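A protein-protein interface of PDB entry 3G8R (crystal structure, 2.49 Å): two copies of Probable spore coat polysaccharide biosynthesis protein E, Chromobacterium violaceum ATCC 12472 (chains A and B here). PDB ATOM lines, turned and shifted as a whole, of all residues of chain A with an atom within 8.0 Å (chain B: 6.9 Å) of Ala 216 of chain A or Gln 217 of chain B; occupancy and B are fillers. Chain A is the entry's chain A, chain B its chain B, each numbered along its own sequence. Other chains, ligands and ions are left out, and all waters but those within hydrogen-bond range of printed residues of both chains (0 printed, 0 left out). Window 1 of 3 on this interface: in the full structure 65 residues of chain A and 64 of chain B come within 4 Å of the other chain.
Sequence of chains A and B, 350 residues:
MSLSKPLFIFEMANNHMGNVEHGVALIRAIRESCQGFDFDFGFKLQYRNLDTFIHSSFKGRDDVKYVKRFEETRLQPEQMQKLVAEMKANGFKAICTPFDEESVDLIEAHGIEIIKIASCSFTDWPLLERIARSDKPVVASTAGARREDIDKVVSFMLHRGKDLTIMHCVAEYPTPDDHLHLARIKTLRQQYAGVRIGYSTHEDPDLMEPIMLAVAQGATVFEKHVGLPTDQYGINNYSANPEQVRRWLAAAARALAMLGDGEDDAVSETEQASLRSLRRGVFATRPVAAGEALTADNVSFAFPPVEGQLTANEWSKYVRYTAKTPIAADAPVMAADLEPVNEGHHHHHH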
ATOM      1  N   ILE A 185      29.742  16.621   5.978  1.00  0.00           N
ATOM      2  CA  ILE A 185      29.442  17.093   7.330  1.00  0.00           C
ATOM      3  C   ILE A 185      30.748  17.140   8.144  1.00  0.00           C
ATOM      4  O   ILE A 185      30.995  18.103   8.877  1.00  0.00           O
ATOM      5  CB  ILE A 185      28.311  16.261   8.021  1.00  0.00           C
ATOM      6  CG1 ILE A 185      27.021  16.286   7.189  1.00  0.00           C
ATOM      7  CG2 ILE A 185      27.948  16.805   9.388  1.00  0.00           C
ATOM      8  CD1 ILE A 185      25.922  15.484   7.798  1.00  0.00           C
ATOM      9  N   LYS A 186      31.596  16.128   7.952  1.00  0.00           N
ATOM     10  CA  LYS A 186      32.867  16.026   8.666  1.00  0.00           C
ATOM     11  C   LYS A 186      33.822  17.037   8.095  1.00  0.00           C
ATOM     12  O   LYS A 186      34.603  17.644   8.839  1.00  0.00           O
ATOM     13  CB  LYS A 186      33.450  14.614   8.580  1.00  0.00           C
ATOM     14  CG  LYS A 186      34.918  14.495   9.029  1.00  0.00           C
ATOM     15  CD  LYS A 186      35.254  13.153   9.688  1.00  0.00           C
ATOM     16  CE  LYS A 186      35.301  11.974   8.691  1.00  0.00           C
ATOM     17  NZ  LYS A 186      34.962  10.619   9.328  1.00  0.00           N
ATOM     18  N   ARG A 189      32.978  20.121   9.706  1.00  0.00           N
ATOM     19  CA  ARG A 189      33.311  20.055  11.129  1.00  0.00           C
ATOM     20  C   ARG A 189      34.804  20.267  11.377  1.00  0.00           C
ATOM     21  O   ARG A 189      35.192  20.969  12.301  1.00  0.00           O
ATOM     22  CB  ARG A 189      32.826  18.749  11.748  1.00  0.00           C
ATOM     23  CG  ARG A 189      33.515  18.421  13.025  1.00  0.00           C
ATOM     24  CD  ARG A 189      32.936  17.169  13.657  1.00  0.00           C
ATOM     25  NE  ARG A 189      31.848  17.417  14.620  1.00  0.00           N
ATOM     26  CZ  ARG A 189      31.467  18.608  15.109  1.00  0.00           C
ATOM     27  NH1 ARG A 189      32.085  19.748  14.750  1.00  0.00           N
ATOM     28  NH2 ARG A 189      30.455  18.652  15.976  1.00  0.00           N
ATOM     29  N   GLU A 209      18.284   6.307   6.792  1.00  0.00           N
ATOM     30  CA  GLU A 209      19.714   6.159   7.105  1.00  0.00           C
ATOM     31  C   GLU A 209      20.537   7.444   7.056  1.00  0.00           C
ATOM     32  O   GLU A 209      21.441   7.598   7.853  1.00  0.00           O
ATOM     33  CB  GLU A 209      20.392   5.048   6.333  1.00  0.00           C
ATOM     34  CG  GLU A 209      20.109   5.066   4.877  1.00  0.00           C
ATOM     35  CD  GLU A 209      19.189   3.941   4.475  1.00  0.00           C
ATOM     36  OE1 GLU A 209      19.658   2.781   4.525  1.00  0.00           O
ATOM     37  OE2 GLU A 209      18.012   4.233   4.114  1.00  0.00           O
ATOM     38  N   PRO A 210      20.231   8.370   6.135  1.00  0.00           N
ATOM     39  CA  PRO A 210      21.064   9.574   6.047  1.00  0.00           C
ATOM     40  C   PRO A 210      21.177  10.298   7.363  1.00  0.00           C
ATOM     41  O   PRO A 210      22.249  10.739   7.710  1.00  0.00           O
ATOM     42  CB  PRO A 210      20.347  10.454   5.016  1.00  0.00           C
ATOM     43  CG  PRO A 210      19.671   9.529   4.131  1.00  0.00           C
ATOM     44  CD  PRO A 210      19.258   8.312   5.028  1.00  0.00           C
ATOM     45  N   ILE A 211      20.089  10.394   8.107  1.00  0.00           N
ATOM     46  CA  ILE A 211      20.129  11.003   9.431  1.00  0.00           C
ATOM     47  C   ILE A 211      21.064  10.270  10.392  1.00  0.00           C
ATOM     48  O   ILE A 211      21.843  10.877  11.111  1.00  0.00           O
ATOM     49  CB  ILE A 211      18.694  11.186   9.994  1.00  0.00           C
ATOM     50  CG1 ILE A 211      18.717  12.216  11.100  1.00  0.00           C
ATOM     51  CG2 ILE A 211      18.028   9.854  10.406  1.00  0.00           C
ATOM     52  CD1 ILE A 211      19.483  13.476  10.714  1.00  0.00           C
ATOM     53  N   MET A 212      21.041   8.954  10.386  1.00  0.00           N
ATOM     54  CA  MET A 212      21.925   8.249  11.276  1.00  0.00           C
ATOM     55  C   MET A 212      23.372   8.575  10.876  1.00  0.00           C
ATOM     56  O   MET A 212      24.208   9.011  11.691  1.00  0.00           O
ATOM     57  CB  MET A 212      21.655   6.761  11.204  1.00  0.00           C
ATOM     58  CG  MET A 212      20.191   6.346  11.196  1.00  0.00           C
ATOM     59  SD  MET A 212      20.096   4.654  11.717  1.00  0.00           S
ATOM     60  CE  MET A 212      18.590   4.185  10.905  1.00  0.00           C
ATOM     61  N   LEU A 213      23.663   8.414   9.597  1.00  0.00           N
ATOM     62  CA  LEU A 213      24.969   8.781   9.063  1.00  0.00           C
ATOM     63  C   LEU A 213      25.329  10.206   9.452  1.00  0.00           C
ATOM     64  O   LEU A 213      26.495  10.520   9.690  1.00  0.00           O
ATOM     65  CB  LEU A 213      24.932   8.643   7.566  1.00  0.00           C
ATOM     66  CG  LEU A 213      25.558   7.380   7.009  1.00  0.00           C
ATOM     67  CD1 LEU A 213      25.197   6.160   7.769  1.00  0.00           C
ATOM     68  CD2 LEU A 213      25.169   7.251   5.564  1.00  0.00           C
ATOM     69  N   ALA A 214      24.310  11.056   9.546  1.00  0.00           N
ATOM     70  CA  ALA A 214      24.534  12.465   9.767  1.00  0.00           C
ATOM     71  C   ALA A 214      24.900  12.669  11.223  1.00  0.00           C
ATOM     72  O   ALA A 214      25.837  13.382  11.547  1.00  0.00           O
ATOM     73  CB  ALA A 214      23.295  13.265   9.398  1.00  0.00           C
ATOM     74  N   VAL A 215      24.159  12.016  12.102  1.00  0.00           N
ATOM     75  CA  VAL A 215      24.416  12.153  13.514  1.00  0.00           C
ATOM     76  C   VAL A 215      25.802  11.652  13.808  1.00  0.00           C
ATOM     77  O   VAL A 215      26.534  12.240  14.613  1.00  0.00           O
ATOM     78  CB  VAL A 215      23.461  11.317  14.288  1.00  0.00           C
ATOM     79  CG1 VAL A 215      23.894  11.267  15.740  1.00  0.00           C
ATOM     80  CG2 VAL A 215      22.096  11.903  14.143  1.00  0.00           C
ATOM     81  N   ALA A 216      26.157  10.573  13.114  1.00  0.00           N
ATOM     82  CA  ALA A 216      27.383   9.834  13.434  1.00  0.00           C
ATOM     83  C   ALA A 216      28.499  10.724  13.102  1.00  0.00           C
ATOM     84  O   ALA A 216      29.550  10.641  13.688  1.00  0.00           O
ATOM     85  CB  ALA A 216      27.505   8.565  12.635  1.00  0.00           C
ATOM     86  N   GLN A 217      28.267  11.605  12.157  1.00  0.00           N
ATOM     87  CA  GLN A 217      29.344  12.420  11.700  1.00  0.00           C
ATOM     88  C   GLN A 217      29.489  13.698  12.531  1.00  0.00           C
ATOM     89  O   GLN A 217      30.335  14.542  12.259  1.00  0.00           O
ATOM     90  CB  GLN A 217      29.163  12.678  10.223  1.00  0.00           C
ATOM     91  CG  GLN A 217      30.464  12.813   9.521  1.00  0.00           C
ATOM     92  CD  GLN A 217      30.426  12.168   8.194  1.00  0.00           C
ATOM     93  OE1 GLN A 217      29.337  12.012   7.614  1.00  0.00           O
ATOM     94  NE2 GLN A 217      31.603  11.759   7.680  1.00  0.00           N
ATOM     95  N   GLY A 218      28.684  13.812  13.579  1.00  0.00           N
ATOM     96  CA  GLY A 218      28.781  14.933  14.503  1.00  0.00           C
ATOM     97  C   GLY A 218      28.015  16.177  14.079  1.00  0.00           C
ATOM     98  O   GLY A 218      28.367  17.273  14.490  1.00  0.00           O
ATOM     99  N   ALA A 219      26.979  16.036  13.259  1.00  0.00           N
ATOM    100  CA  ALA A 219      26.017  17.124  13.095  1.00  0.00           C
ATOM    101  C   ALA A 219      25.012  17.141  14.254  1.00  0.00           C
ATOM    102  O   ALA A 219      24.675  16.098  14.804  1.00  0.00           O
ATOM    103  CB  ALA A 219      25.314  17.004  11.799  1.00  0.00           C
ATOM    104  N   PHE A 222      19.394  19.705  12.474  1.00  0.00           N
ATOM    105  CA  PHE A 222      18.918  18.911  11.364  1.00  0.00           C
ATOM    106  C   PHE A 222      17.696  19.554  10.822  1.00  0.00           C
ATOM    107  O   PHE A 222      16.782  19.841  11.565  1.00  0.00           O
ATOM    108  CB  PHE A 222      18.612  17.499  11.856  1.00  0.00           C
ATOM    109  CG  PHE A 222      19.821  16.783  12.417  1.00  0.00           C
ATOM    110  CD1 PHE A 222      20.736  16.158  11.569  1.00  0.00           C
ATOM    111  CD2 PHE A 222      20.065  16.763  13.791  1.00  0.00           C
ATOM    112  CE1 PHE A 222      21.876  15.518  12.083  1.00  0.00           C
ATOM    113  CE2 PHE A 222      21.178  16.129  14.320  1.00  0.00           C
ATOM    114  CZ  PHE A 222      22.093  15.505  13.471  1.00  0.00           C
ATOM    115  N   ALA A 255      20.114   5.841  16.391  1.00  0.00           N
ATOM    116  CA  ALA A 255      21.517   6.077  16.100  1.00  0.00           C
ATOM    117  C   ALA A 255      22.243   6.595  17.331  1.00  0.00           C
ATOM    118  O   ALA A 255      23.396   6.250  17.555  1.00  0.00           O
ATOM    119  CB  ALA A 255      21.639   7.091  14.988  1.00  0.00           C
ATOM    120  N   LEU A 256      21.558   7.398  18.148  1.00  0.00           N
ATOM    121  CA  LEU A 256      22.191   7.911  19.334  1.00  0.00           C
ATOM    122  C   LEU A 256      22.441   6.783  20.302  1.00  0.00           C
ATOM    123  O   LEU A 256      23.493   6.732  20.941  1.00  0.00           O
ATOM    124  CB  LEU A 256      21.346   8.997  19.973  1.00  0.00           C
ATOM    125  CG  LEU A 256      21.268  10.257  19.111  1.00  0.00           C
ATOM    126  CD1 LEU A 256      20.075  11.063  19.481  1.00  0.00           C
ATOM    127  CD2 LEU A 256      22.526  11.076  19.140  1.00  0.00           C
ATOM    128  N   MET A 258      22.706   3.503  19.682  1.00  0.00           N
ATOM    129  CA  MET A 258      23.739   2.668  19.112  1.00  0.00           C
ATOM    130  C   MET A 258      25.098   3.358  19.223  1.00  0.00           C
ATOM    131  O   MET A 258      26.102   2.697  19.226  1.00  0.00           O
ATOM    132  CB  MET A 258      23.441   2.392  17.632  1.00  0.00           C
ATOM    133  CG  MET A 258      22.589   1.198  17.332  1.00  0.00           C
ATOM    134  SD  MET A 258      22.264   1.060  15.567  1.00  0.00           S
ATOM    135  CE  MET A 258      21.694  -0.575  15.763  1.00  0.00           C
ATOM    136  N   LEU A 259      25.139   4.682  19.266  1.00  0.00           N
ATOM    137  CA  LEU A 259      26.411   5.369  19.253  1.00  0.00           C
ATOM    138  C   LEU A 259      27.001   5.435  20.647  1.00  0.00           C
ATOM    139  O   LEU A 259      28.233   5.478  20.820  1.00  0.00           O
ATOM    140  CB  LEU A 259      26.275   6.769  18.638  1.00  0.00           C
ATOM    141  CG  LEU A 259      26.348   6.882  17.087  1.00  0.00           C
ATOM    142  CD1 LEU A 259      25.954   8.231  16.603  1.00  0.00           C
ATOM    143  CD2 LEU A 259      27.700   6.574  16.507  1.00  0.00           C
ATOM    144  N   GLY A 260      26.120   5.447  21.645  1.00  0.00           N
ATOM    145  CA  GLY A 260      26.519   5.709  23.013  1.00  0.00           C
ATOM    146  C   GLY A 260      27.263   6.999  23.122  1.00  0.00           C
ATOM    147  O   GLY A 260      27.205   7.811  22.235  1.00  0.00           O
ATOM    148  N   GLY A 262      30.877   8.920  23.384  1.00  0.00           N
ATOM    149  CA  GLY A 262      32.297   8.735  23.052  1.00  0.00           C
ATOM    150  C   GLY A 262      33.218   9.104  24.204  1.00  0.00           C
ATOM    151  O   GLY A 262      34.408   8.804  24.197  1.00  0.00           O
ATOM    152  N   HIS B 181      28.155   0.985  21.558  1.00  0.00           N
ATOM    153  CA  HIS B 181      29.065   2.051  21.804  1.00  0.00           C
ATOM    154  C   HIS B 181      29.859   2.466  20.556  1.00  0.00           C
ATOM    155  O   HIS B 181      31.052   2.749  20.650  1.00  0.00           O
ATOM    156  CB  HIS B 181      29.969   1.656  22.945  1.00  0.00           C
ATOM    157  CG  HIS B 181      30.597   2.813  23.644  1.00  0.00           C
ATOM    158  ND1 HIS B 181      31.627   2.662  24.551  1.00  0.00           N
ATOM    159  CD2 HIS B 181      30.370   4.144  23.544  1.00  0.00           C
ATOM    160  CE1 HIS B 181      31.992   3.853  24.996  1.00  0.00           C
ATOM    161  NE2 HIS B 181      31.251   4.769  24.395  1.00  0.00           N
ATOM    162  N   LEU B 182      29.188   2.580  19.403  1.00  0.00           N
ATOM    163  CA  LEU B 182      29.906   2.834  18.111  1.00  0.00           C
ATOM    164  C   LEU B 182      30.791   4.089  18.053  1.00  0.00           C
ATOM    165  O   LEU B 182      31.641   4.196  17.181  1.00  0.00           O
ATOM    166  CB  LEU B 182      28.953   2.805  16.898  1.00  0.00           C
ATOM    167  CG  LEU B 182      28.296   1.437  16.659  1.00  0.00           C
ATOM    168  CD1 LEU B 182      27.373   1.451  15.470  1.00  0.00           C
ATOM    169  CD2 LEU B 182      29.314   0.325  16.463  1.00  0.00           C
ATOM    170  N   ALA B 183      30.579   5.025  18.975  1.00  0.00           N
ATOM    171  CA  ALA B 183      31.305   6.279  18.985  1.00  0.00           C
ATOM    172  C   ALA B 183      32.679   6.108  19.550  1.00  0.00           C
ATOM    173  O   ALA B 183      33.443   7.044  19.578  1.00  0.00           O
ATOM    174  CB  ALA B 183      30.571   7.310  19.795  1.00  0.00           C
ATOM    175  N   ARG B 184      33.013   4.922  20.025  1.00  0.00           N
ATOM    176  CA  ARG B 184      34.399   4.716  20.393  1.00  0.00           C
ATOM    177  C   ARG B 184      35.248   4.748  19.110  1.00  0.00           C
ATOM    178  O   ARG B 184      36.387   5.182  19.131  1.00  0.00           O
ATOM    179  CB  ARG B 184      34.590   3.442  21.208  1.00  0.00           C
ATOM    180  CG  ARG B 184      35.685   3.633  22.213  1.00  0.00           C
ATOM    181  CD  ARG B 184      35.652   2.595  23.276  1.00  0.00           C
ATOM    182  NE  ARG B 184      36.235   1.338  22.810  1.00  0.00           N
ATOM    183  CZ  ARG B 184      37.361   0.783  23.269  1.00  0.00           C
ATOM    184  NH1 ARG B 184      38.076   1.340  24.252  1.00  0.00           N
ATOM    185  NH2 ARG B 184      37.744  -0.359  22.737  1.00  0.00           N
ATOM    186  N   ILE B 185      34.657   4.346  17.994  1.00  0.00           N
ATOM    187  CA  ILE B 185      35.299   4.501  16.733  1.00  0.00           C
ATOM    188  C   ILE B 185      35.832   5.904  16.537  1.00  0.00           C
ATOM    189  O   ILE B 185      37.005   6.060  16.202  1.00  0.00           O
ATOM    190  CB  ILE B 185      34.403   4.131  15.586  1.00  0.00           C
ATOM    191  CG1 ILE B 185      33.900   2.701  15.792  1.00  0.00           C
ATOM    192  CG2 ILE B 185      35.177   4.293  14.241  1.00  0.00           C
ATOM    193  CD1 ILE B 185      33.163   2.153  14.576  1.00  0.00           C
ATOM    194  N   LYS B 186      35.011   6.924  16.779  1.00  0.00           N
ATOM    195  CA  LYS B 186      35.519   8.288  16.635  1.00  0.00           C
ATOM    196  C   LYS B 186      36.557   8.583  17.717  1.00  0.00           C
ATOM    197  O   LYS B 186      37.639   9.077  17.429  1.00  0.00           O
ATOM    198  CB  LYS B 186      34.405   9.329  16.674  1.00  0.00           C
ATOM    199  CG  LYS B 186      34.886  10.753  16.471  1.00  0.00           C
ATOM    200  CD  LYS B 186      33.723  11.680  16.143  1.00  0.00           C
ATOM    201  CE  LYS B 186      33.028  11.290  14.799  1.00  0.00           C
ATOM    202  NZ  LYS B 186      31.944  12.254  14.352  1.00  0.00           N
ATOM    203  N   THR B 187      36.236   8.244  18.961  1.00  0.00           N
ATOM    204  CA  THR B 187      37.161   8.511  20.034  1.00  0.00           C
ATOM    205  C   THR B 187      38.537   8.014  19.652  1.00  0.00           C
ATOM    206  O   THR B 187      39.508   8.756  19.722  1.00  0.00           O
ATOM    207  CB  THR B 187      36.696   7.855  21.304  1.00  0.00           C
ATOM    208  OG1 THR B 187      35.554   8.568  21.787  1.00  0.00           O
ATOM    209  CG2 THR B 187      37.793   7.866  22.374  1.00  0.00           C
ATOM    210  N   ARG B 189      39.771   7.252  16.756  1.00  0.00           N
ATOM    211  CA  ARG B 189      40.378   7.876  15.588  1.00  0.00           C
ATOM    212  C   ARG B 189      41.073   9.124  16.100  1.00  0.00           C
ATOM    213  O   ARG B 189      42.199   9.424  15.729  1.00  0.00           O
ATOM    214  CB  ARG B 189      39.330   8.221  14.515  1.00  0.00           C
ATOM    215  CG  ARG B 189      39.729   7.792  13.080  1.00  0.00           C
ATOM    216  CD  ARG B 189      39.243   8.758  11.988  1.00  0.00           C
ATOM    217  NE  ARG B 189      38.976   8.082  10.712  1.00  0.00           N
ATOM    218  CZ  ARG B 189      39.662   8.279   9.582  1.00  0.00           C
ATOM    219  NH1 ARG B 189      40.673   9.149   9.549  1.00  0.00           N
ATOM    220  NH2 ARG B 189      39.327   7.608   8.478  1.00  0.00           N
ATOM    221  N   ILE B 197      41.807   2.620  11.938  1.00  0.00           N
ATOM    222  CA  ILE B 197      40.796   2.139  12.871  1.00  0.00           C
ATOM    223  C   ILE B 197      39.777   1.220  12.220  1.00  0.00           C
ATOM    224  O   ILE B 197      39.269   1.486  11.149  1.00  0.00           O
ATOM    225  CB  ILE B 197      40.000   3.314  13.499  1.00  0.00           C
ATOM    226  CG1 ILE B 197      40.950   4.392  14.065  1.00  0.00           C
ATOM    227  CG2 ILE B 197      39.078   2.803  14.586  1.00  0.00           C
ATOM    228  CD1 ILE B 197      41.929   3.871  15.128  1.00  0.00           C
ATOM    229  N   PRO B 210      24.696  -0.627  12.090  1.00  0.00           N
ATOM    230  CA  PRO B 210      25.954  -0.304  12.764  1.00  0.00           C
ATOM    231  C   PRO B 210      27.109  -0.209  11.819  1.00  0.00           C
ATOM    232  O   PRO B 210      27.913   0.701  11.954  1.00  0.00           O
ATOM    233  CB  PRO B 210      26.142  -1.470  13.722  1.00  0.00           C
ATOM    234  CG  PRO B 210      24.735  -1.857  14.081  1.00  0.00           C
ATOM    235  CD  PRO B 210      24.024  -1.765  12.757  1.00  0.00           C
ATOM    236  N   ILE B 211      27.189  -1.091  10.831  1.00  0.00           N
ATOM    237  CA  ILE B 211      28.266  -0.932   9.861  1.00  0.00           C
ATOM    238  C   ILE B 211      28.229   0.407   9.116  1.00  0.00           C
ATOM    239  O   ILE B 211      29.271   1.057   8.907  1.00  0.00           O
ATOM    240  CB  ILE B 211      28.422  -2.129   8.894  1.00  0.00           C
ATOM    241  CG1 ILE B 211      29.784  -1.981   8.260  1.00  0.00           C
ATOM    242  CG2 ILE B 211      27.278  -2.189   7.852  1.00  0.00           C
ATOM    243  CD1 ILE B 211      30.410  -3.224   7.769  1.00  0.00           C
ATOM    244  N   MET B 212      27.029   0.825   8.732  1.00  0.00           N
ATOM    245  CA  MET B 212      26.850   2.142   8.120  1.00  0.00           C
ATOM    246  C   MET B 212      27.392   3.228   9.049  1.00  0.00           C
ATOM    247  O   MET B 212      28.026   4.183   8.584  1.00  0.00           O
ATOM    248  CB  MET B 212      25.387   2.420   7.762  1.00  0.00           C
ATOM    249  CG  MET B 212      24.713   1.297   6.965  1.00  0.00           C
ATOM    250  SD  MET B 212      23.205   1.833   6.210  1.00  0.00           S
ATOM    251  CE  MET B 212      23.864   2.776   4.906  1.00  0.00           C
ATOM    252  N   LEU B 213      27.170   3.065  10.351  1.00  0.00           N
ATOM    253  CA  LEU B 213      27.663   4.021  11.353  1.00  0.00           C
ATOM    254  C   LEU B 213      29.198   3.922  11.535  1.00  0.00           C
ATOM    255  O   LEU B 213      29.911   4.921  11.622  1.00  0.00           O
ATOM    256  CB  LEU B 213      26.956   3.761  12.704  1.00  0.00           C
ATOM    257  CG  LEU B 213      25.635   4.467  12.931  1.00  0.00           C
ATOM    258  CD1 LEU B 213      24.881   4.717  11.656  1.00  0.00           C
ATOM    259  CD2 LEU B 213      24.725   3.729  13.934  1.00  0.00           C
ATOM    260  N   ALA B 214      29.685   2.695  11.618  1.00  0.00           N
ATOM    261  CA  ALA B 214      31.109   2.442  11.669  1.00  0.00           C
ATOM    262  C   ALA B 214      31.800   3.205  10.554  1.00  0.00           C
ATOM    263  O   ALA B 214      32.776   3.947  10.763  1.00  0.00           O
ATOM    264  CB  ALA B 214      31.407   0.907  11.528  1.00  0.00           C
ATOM    265  N   VAL B 215      31.269   3.007   9.367  1.00  0.00           N
ATOM    266  CA  VAL B 215      31.911   3.515   8.187  1.00  0.00           C
ATOM    267  C   VAL B 215      31.887   5.032   8.244  1.00  0.00           C
ATOM    268  O   VAL B 215      32.881   5.700   7.880  1.00  0.00           O
ATOM    269  CB  VAL B 215      31.170   3.035   6.932  1.00  0.00           C
ATOM    270  CG1 VAL B 215      31.382   3.961   5.844  1.00  0.00           C
ATOM    271  CG2 VAL B 215      31.664   1.723   6.548  1.00  0.00           C
ATOM    272  N   ALA B 216      30.759   5.566   8.704  1.00  0.00           N
ATOM    273  CA  ALA B 216      30.615   7.023   8.754  1.00  0.00           C
ATOM    274  C   ALA B 216      31.606   7.659   9.736  1.00  0.00           C
ATOM    275  O   ALA B 216      31.945   8.837   9.612  1.00  0.00           O
ATOM    276  CB  ALA B 216      29.190   7.423   9.091  1.00  0.00           C
ATOM    277  N   GLN B 217      32.071   6.887  10.715  1.00  0.00           N
ATOM    278  CA  GLN B 217      33.077   7.430  11.618  1.00  0.00           C
ATOM    279  C   GLN B 217      34.505   7.195  11.157  1.00  0.00           C
ATOM    280  O   GLN B 217      35.468   7.612  11.814  1.00  0.00           O
ATOM    281  CB  GLN B 217      32.826   6.977  13.033  1.00  0.00           C
ATOM    282  CG  GLN B 217      31.672   7.718  13.569  1.00  0.00           C
ATOM    283  CD  GLN B 217      31.323   7.274  14.908  1.00  0.00           C
ATOM    284  OE1 GLN B 217      31.416   8.029  15.884  1.00  0.00           O
ATOM    285  NE2 GLN B 217      30.918   6.027  14.995  1.00  0.00           N
ATOM    286  N   GLY B 218      34.620   6.566   9.994  1.00  0.00           N
ATOM    287  CA  GLY B 218      35.890   6.429   9.335  1.00  0.00           C
ATOM    288  C   GLY B 218      36.633   5.203   9.789  1.00  0.00           C
ATOM    289  O   GLY B 218      37.855   5.213   9.808  1.00  0.00           O
ATOM    290  N   ALA B 219      35.909   4.142  10.139  1.00  0.00           N
ATOM    291  CA  ALA B 219      36.530   2.828  10.293  1.00  0.00           C
ATOM    292  C   ALA B 219      36.846   2.364   8.881  1.00  0.00           C
ATOM    293  O   ALA B 219      36.172   2.767   7.947  1.00  0.00           O
ATOM    294  CB  ALA B 219      35.586   1.862  10.978  1.00  0.00           C
ATOM    295  N   LEU B 259      27.721   8.624   1.615  1.00  0.00           N
ATOM    296  CA  LEU B 259      28.731   9.509   2.137  1.00  0.00           C
ATOM    297  C   LEU B 259      29.472  10.290   1.061  1.00  0.00           C
ATOM    298  O   LEU B 259      29.749  11.469   1.252  1.00  0.00           O
ATOM    299  CB  LEU B 259      29.750   8.697   2.936  1.00  0.00           C
ATOM    300  CG  LEU B 259      29.426   8.497   4.403  1.00  0.00           C
ATOM    301  CD1 LEU B 259      30.439   7.551   5.001  1.00  0.00           C
ATOM    302  CD2 LEU B 259      29.474   9.817   5.118  1.00  0.00           C
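Met 212 of chain A touches Leu 213 of chain B, and with the chains exchanged Leu 213 of chain A touches Met 212 of chain B.
Ala 216 of chain A touches Gln 217 of chain B, and with the chains exchanged Gln 217 of chain A touches Ala 216 of chain B.
Of the 20 printed residues of chain B, 11 touch a printed residue of chain A.
Printed residues of chain B that touch a printed residue of chain A: His 181, Leu 182, Ala 183, Lys 186, Thr 187, Pro 210, Met 212, Leu 213, Ala 216, Gln 217 and Leu 259.
Hydrophobic or aromatic side chains of chain B within 4 Å of the printed part of chain A: His 181, Leu 182, Ala 183, Pro 210, Met 212, Leu 213 and Leu 259.
Of the 21 printed residues of chain A, 9 touch a printed residue of chain B.
Hydrophobic or aromatic side chains of chain A within 4 Å of the printed part of chain B: Met 212, Leu 213, Met 258 and Leu 259.
Among the printed residues, no Asp or Glu carboxylate lies within 4 Å of a Lys or Arg side-chain nitrogen of the other chain.
Of the printed residues of chain B, Lys 186 of chain A touches Ala 216 (3.5 Å) and Gln 217 (3.9 Å).
Ile 211 of chain A touches none of the printed residues of chain B.
Of the printed residues of chain B, Met 212 of chain A touches Leu 213.
Ala 216 of chain A touches just these residues of chain B: Lys 186 and Gln 217.
Of the printed residues of chain A, Met 212 of chain B touches Leu 213.
The backbone carbonyl oxygen (O) of Ala 216 of chain A lies within hydrogen-bond range of the side-chain amino group (NZ) of Lys 186 of chain B (3.0 Å).
The side-chain amino group (NZ) of Lys 186 of chain B lies close to the backbone carbonyl oxygen (O) of Gln 217 of chain A, at 3.5 Å.
The backbone carbonyl oxygen of Met 258 of chain A is in hydrogen-bond range of the backbone NH of Leu 182 of chain B (3.1 Å).
The backbone carbonyl oxygen (O) of Leu 259 of chain A lies within hydrogen-bond range of the backbone NH (N) of Leu 182 of chain B (3.4 Å).
The backbone carbonyl oxygen (O) of Leu 259 of chain A is in hydrogen-bond range of the backbone NH (N) of Ala 183 of chain B (3.0 Å).
The backbone carbonyl oxygen (O) of Gly 262 of chain A lies within hydrogen-bond range of the side-chain hydroxyl (OG1) of Thr 187 of chain B, 2.7 Å away.
NE2 of Gln 217 of chain B sits at hydrogen-bond distance from O of Leu 182 of chain B, at 2.9 Å.
The backbone carbonyl oxygen (O) of Ala 183 of chain B is in hydrogen-bond range of the side-chain hydroxyl (OG1) of Thr 187 of chain B, at 3.4 Å.
Lys 186 of chain A touches Gln 217 of chain B.
Leu 213 of chain A touches Met 212 of chain B (CD1 to O, 3.5 Å).
Gln 217 of chain A touches Ala 216 of chain B (NE2 to O, 3.5 Å).
Gln 217 of chain A touches Leu 259 of chain B (OE1 to CD2, 3.3 Å).
Gly 218 of chain A touches Lys 186 of chain B (N to NZ, 3.7 Å).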
